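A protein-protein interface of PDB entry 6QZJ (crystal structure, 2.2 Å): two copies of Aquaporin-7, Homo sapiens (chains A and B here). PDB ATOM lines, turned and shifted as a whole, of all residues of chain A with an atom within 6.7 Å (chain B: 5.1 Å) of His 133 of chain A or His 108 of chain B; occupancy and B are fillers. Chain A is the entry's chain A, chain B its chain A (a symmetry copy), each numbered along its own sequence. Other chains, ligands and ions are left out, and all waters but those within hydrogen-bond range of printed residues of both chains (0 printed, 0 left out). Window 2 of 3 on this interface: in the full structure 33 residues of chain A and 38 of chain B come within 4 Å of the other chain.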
ATOM      1  N   LEU A 130      33.163  27.564  15.602  1.00  0.00           N
ATOM      2  CA  LEU A 130      32.886  26.466  16.511  1.00  0.00           C
ATOM      3  C   LEU A 130      31.413  26.071  16.428  1.00  0.00           C
ATOM      4  O   LEU A 130      30.544  26.935  16.275  1.00  0.00           O
ATOM      5  CB  LEU A 130      33.264  26.834  17.948  1.00  0.00           C
ATOM      6  CG  LEU A 130      32.548  27.975  18.661  1.00  0.00           C
ATOM      7  CD1 LEU A 130      32.602  27.761  20.162  1.00  0.00           C
ATOM      8  CD2 LEU A 130      33.181  29.300  18.297  1.00  0.00           C
ATOM      9  N   PRO A 131      31.104  24.780  16.510  1.00  0.00           N
ATOM     10  CA  PRO A 131      29.712  24.342  16.380  1.00  0.00           C
ATOM     11  C   PRO A 131      28.861  24.869  17.522  1.00  0.00           C
ATOM     12  O   PRO A 131      29.351  25.370  18.536  1.00  0.00           O
ATOM     13  CB  PRO A 131      29.808  22.814  16.412  1.00  0.00           C
ATOM     14  CG  PRO A 131      31.096  22.534  17.115  1.00  0.00           C
ATOM     15  CD  PRO A 131      32.021  23.652  16.745  1.00  0.00           C
ATOM     16  N   ASP A 132      27.547  24.742  17.333  1.00  0.00           N
ATOM     17  CA  ASP A 132      26.591  25.284  18.290  1.00  0.00           C
ATOM     18  C   ASP A 132      26.628  24.564  19.630  1.00  0.00           C
ATOM     19  O   ASP A 132      26.246  25.156  20.645  1.00  0.00           O
ATOM     20  CB  ASP A 132      25.184  25.215  17.702  1.00  0.00           C
ATOM     21  CG  ASP A 132      25.109  25.812  16.314  1.00  0.00           C
ATOM     22  OD1 ASP A 132      25.343  27.032  16.180  1.00  0.00           O
ATOM     23  OD2 ASP A 132      24.816  25.064  15.357  1.00  0.00           O
ATOM     24  N   HIS A 133      27.075  23.311  19.663  1.00  0.00           N
ATOM     25  CA  HIS A 133      27.089  22.550  20.906  1.00  0.00           C
ATOM     26  C   HIS A 133      28.269  22.894  21.803  1.00  0.00           C
ATOM     27  O   HIS A 133      28.379  22.326  22.894  1.00  0.00           O
ATOM     28  CB  HIS A 133      27.077  21.044  20.605  1.00  0.00           C
ATOM     29  CG  HIS A 133      28.320  20.540  19.940  1.00  0.00           C
ATOM     30  ND1 HIS A 133      29.498  20.327  20.621  1.00  0.00           N
ATOM     31  CD2 HIS A 133      28.562  20.190  18.654  1.00  0.00           C
ATOM     32  CE1 HIS A 133      30.415  19.875  19.783  1.00  0.00           C
ATOM     33  NE2 HIS A 133      29.872  19.785  18.582  1.00  0.00           N
ATOM     34  N   MET A 134      29.129  23.819  21.389  1.00  0.00           N
ATOM     35  CA  MET A 134      30.383  24.105  22.069  1.00  0.00           C
ATOM     36  C   MET A 134      30.314  25.429  22.820  1.00  0.00           C
ATOM     37  O   MET A 134      29.494  26.301  22.521  1.00  0.00           O
ATOM     38  CB  MET A 134      31.542  24.142  21.068  1.00  0.00           C
ATOM     39  CG  MET A 134      32.044  22.773  20.667  1.00  0.00           C
ATOM     40  SD  MET A 134      33.021  22.028  21.980  1.00  0.00           S
ATOM     41  CE  MET A 134      34.374  23.193  22.081  1.00  0.00           C
ATOM     42  N   THR A 135      31.192  25.565  23.809  1.00  0.00           N
ATOM     43  CA  THR A 135      31.407  26.815  24.521  1.00  0.00           C
ATOM     44  C   THR A 135      32.785  27.366  24.177  1.00  0.00           C
ATOM     45  O   THR A 135      33.683  26.629  23.755  1.00  0.00           O
ATOM     46  CB  THR A 135      31.277  26.623  26.039  1.00  0.00           C
ATOM     47  OG1 THR A 135      32.468  26.016  26.554  1.00  0.00           O
ATOM     48  CG2 THR A 135      30.083  25.740  26.369  1.00  0.00           C
ATOM     49  N   MET A 187      36.372  17.602  15.206  1.00  0.00           N
ATOM     50  CA  MET A 187      34.957  17.967  15.108  1.00  0.00           C
ATOM     51  C   MET A 187      34.590  19.113  16.042  1.00  0.00           C
ATOM     52  O   MET A 187      33.731  19.931  15.697  1.00  0.00           O
ATOM     53  CB  MET A 187      34.068  16.752  15.386  1.00  0.00           C
ATOM     54  CG  MET A 187      34.156  16.199  16.800  1.00  0.00           C
ATOM     55  SD  MET A 187      32.654  15.322  17.283  1.00  0.00           S
ATOM     56  CE  MET A 187      32.473  14.221  15.889  1.00  0.00           C
ATOM     57  N   ASN A 188      35.233  19.210  17.206  1.00  0.00           N
ATOM     58  CA  ASN A 188      34.761  20.133  18.230  1.00  0.00           C
ATOM     59  C   ASN A 188      35.145  21.580  17.958  1.00  0.00           C
ATOM     60  O   ASN A 188      34.541  22.486  18.543  1.00  0.00           O
ATOM     61  CB  ASN A 188      35.293  19.722  19.604  1.00  0.00           C
ATOM     62  CG  ASN A 188      34.795  18.359  20.037  1.00  0.00           C
ATOM     63  OD1 ASN A 188      33.597  18.090  20.007  1.00  0.00           O
ATOM     64  ND2 ASN A 188      35.716  17.490  20.447  1.00  0.00           N
ATOM     65  N   THR A 189      36.118  21.823  17.086  1.00  0.00           N
ATOM     66  CA  THR A 189      36.643  23.173  16.927  1.00  0.00           C
ATOM     67  C   THR A 189      37.186  23.391  15.517  1.00  0.00           C
ATOM     68  O   THR A 189      37.487  24.523  15.119  1.00  0.00           O
ATOM     69  CB  THR A 189      37.728  23.418  17.985  1.00  0.00           C
ATOM     70  OG1 THR A 189      37.175  23.230  19.295  1.00  0.00           O
ATOM     71  CG2 THR A 189      38.283  24.815  17.901  1.00  0.00           C
ATOM     72  N   TYR B 103      33.118  16.928  26.007  1.00  0.00           N
ATOM     73  CA  TYR B 103      32.100  16.966  27.056  1.00  0.00           C
ATOM     74  C   TYR B 103      30.755  17.461  26.542  1.00  0.00           C
ATOM     75  O   TYR B 103      29.777  16.705  26.529  1.00  0.00           O
ATOM     76  CB  TYR B 103      32.563  17.841  28.227  1.00  0.00           C
ATOM     77  CG  TYR B 103      31.600  17.852  29.395  1.00  0.00           C
ATOM     78  CD1 TYR B 103      31.200  16.666  30.002  1.00  0.00           C
ATOM     79  CD2 TYR B 103      31.084  19.044  29.886  1.00  0.00           C
ATOM     80  CE1 TYR B 103      30.309  16.669  31.071  1.00  0.00           C
ATOM     81  CE2 TYR B 103      30.194  19.057  30.953  1.00  0.00           C
ATOM     82  CZ  TYR B 103      29.812  17.868  31.542  1.00  0.00           C
ATOM     83  OH  TYR B 103      28.930  17.877  32.600  1.00  0.00           O
ATOM     84  N   THR B 104      30.692  18.725  26.115  1.00  0.00           N
ATOM     85  CA  THR B 104      29.431  19.264  25.616  1.00  0.00           C
ATOM     86  C   THR B 104      28.982  18.571  24.335  1.00  0.00           C
ATOM     87  O   THR B 104      27.779  18.528  24.047  1.00  0.00           O
ATOM     88  CB  THR B 104      29.550  20.769  25.385  1.00  0.00           C
ATOM     89  OG1 THR B 104      30.364  21.014  24.233  1.00  0.00           O
ATOM     90  CG2 THR B 104      30.147  21.456  26.603  1.00  0.00           C
ATOM     91  N   ALA B 105      29.919  18.034  23.553  1.00  0.00           N
ATOM     92  CA  ALA B 105      29.531  17.251  22.385  1.00  0.00           C
ATOM     93  C   ALA B 105      28.782  15.992  22.800  1.00  0.00           C
ATOM     94  O   ALA B 105      27.761  15.637  22.197  1.00  0.00           O
ATOM     95  CB  ALA B 105      30.764  16.899  21.555  1.00  0.00           C
ATOM     96  N   ILE B 106      29.268  15.311  23.838  1.00  0.00           N
ATOM     97  CA  ILE B 106      28.563  14.142  24.354  1.00  0.00           C
ATOM     98  C   ILE B 106      27.260  14.564  25.021  1.00  0.00           C
ATOM     99  O   ILE B 106      26.232  13.887  24.889  1.00  0.00           O
ATOM    100  CB  ILE B 106      29.470  13.354  25.317  1.00  0.00           C
ATOM    101  CG1 ILE B 106      30.685  12.785  24.575  1.00  0.00           C
ATOM    102  CG2 ILE B 106      28.700  12.228  25.991  1.00  0.00           C
ATOM    103  CD1 ILE B 106      31.698  12.124  25.477  1.00  0.00           C
ATOM    104  N   LEU B 107      27.274  15.695  25.732  1.00  0.00           N
ATOM    105  CA  LEU B 107      26.071  16.165  26.414  1.00  0.00           C
ATOM    106  C   LEU B 107      24.984  16.552  25.421  1.00  0.00           C
ATOM    107  O   LEU B 107      23.833  16.120  25.549  1.00  0.00           O
ATOM    108  CB  LEU B 107      26.406  17.350  27.320  1.00  0.00           C
ATOM    109  CG  LEU B 107      27.114  17.051  28.643  1.00  0.00           C
ATOM    110  CD1 LEU B 107      26.901  18.200  29.620  1.00  0.00           C
ATOM    111  CD2 LEU B 107      26.632  15.734  29.236  1.00  0.00           C
ATOM    112  N   HIS B 108      25.326  17.379  24.430  1.00  0.00           N
ATOM    113  CA  HIS B 108      24.327  17.814  23.458  1.00  0.00           C
ATOM    114  C   HIS B 108      23.806  16.639  22.640  1.00  0.00           C
ATOM    115  O   HIS B 108      22.610  16.565  22.334  1.00  0.00           O
ATOM    116  CB  HIS B 108      24.918  18.890  22.547  1.00  0.00           C
ATOM    117  CG  HIS B 108      24.246  18.991  21.212  1.00  0.00           C
ATOM    118  ND1 HIS B 108      24.688  18.302  20.103  1.00  0.00           N
ATOM    119  CD2 HIS B 108      23.165  19.701  20.808  1.00  0.00           C
ATOM    120  CE1 HIS B 108      23.909  18.582  19.074  1.00  0.00           C
ATOM    121  NE2 HIS B 108      22.978  19.429  19.475  1.00  0.00           N
ATOM    122  N   PHE B 109      24.692  15.706  22.280  1.00  0.00           N
ATOM    123  CA  PHE B 109      24.266  14.510  21.558  1.00  0.00           C
ATOM    124  C   PHE B 109      23.333  13.657  22.409  1.00  0.00           C
ATOM    125  O   PHE B 109      22.312  13.159  21.919  1.00  0.00           O
ATOM    126  CB  PHE B 109      25.495  13.709  21.121  1.00  0.00           C
ATOM    127  CG  PHE B 109      25.188  12.313  20.642  1.00  0.00           C
ATOM    128  CD1 PHE B 109      24.713  12.093  19.356  1.00  0.00           C
ATOM    129  CD2 PHE B 109      25.406  11.220  21.465  1.00  0.00           C
ATOM    130  CE1 PHE B 109      24.445  10.813  18.909  1.00  0.00           C
ATOM    131  CE2 PHE B 109      25.139   9.939  21.024  1.00  0.00           C
ATOM    132  CZ  PHE B 109      24.659   9.737  19.744  1.00  0.00           C
ATOM    133  N   SER B 110      23.656  13.494  23.691  1.00  0.00           N
ATOM    134  CA  SER B 110      22.900  12.634  24.589  1.00  0.00           C
ATOM    135  C   SER B 110      21.864  13.383  25.420  1.00  0.00           C
ATOM    136  O   SER B 110      21.149  12.750  26.206  1.00  0.00           O
ATOM    137  CB  SER B 110      23.866  11.865  25.502  1.00  0.00           C
ATOM    138  OG  SER B 110      24.102  12.546  26.722  1.00  0.00           O
ATOM    139  N   GLY B 111      21.741  14.698  25.252  1.00  0.00           N
ATOM    140  CA  GLY B 111      20.791  15.463  26.034  1.00  0.00           C
ATOM    141  C   GLY B 111      21.100  15.533  27.511  1.00  0.00           C
ATOM    142  O   GLY B 111      20.257  15.996  28.284  1.00  0.00           O
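His 133 of chain A touches Ala 105 of chain B (CE1 to CB, 3.5 Å). CB of His 133 of chain A touches CG of His 108 of chain B, 3.5 Å away. Ala 105 of chain B touches Asn 188 of chain A (CB to OD1, 3.4 Å).
Of the 9 printed residues of chain A, 3 touch a printed residue of chain B. Among the printed residues, 5 pairs touch across the chains. Among the printed residues, no Asp or Glu carboxylate lies within 4 Å of a Lys or Arg side-chain nitrogen of the other chain.
The side-chain hydroxyl of Thr 104 of chain B is in hydrogen-bond range of the side-chain sulfur of Met 134 of chain A, 3.6 Å away. OG1 of Thr 104 of chain B is in hydrogen-bond range of O of His 133 of chain A.
No position is printed for both chains. Of the 5 pairs that touch across the chains among the printed residues, none has its exchanged pair printed and touching as well.
Of chain B, only Thr 104 (2.7 Å), Ala 105 (3.5 Å) and His 108 (3.5 Å) come within 4 Å of His 133 of chain A. Of the printed residues of chain B, Met 134 of chain A touches Thr 104. Printed residues of chain B within 4 Å of Asn 188 of chain A: Ala 105. Printed residues of chain A within 4 Å of Thr 104 of chain B: His 133 and Met 134. Ile 106 of chain B touches none of the printed residues of chain A. Of chain A, only His 133 comes within 4 Å of His 108 of chain B. The nearest residue of chain A that does not touch His 108 of chain B is Asp 132 of chain A (6.1 Å).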
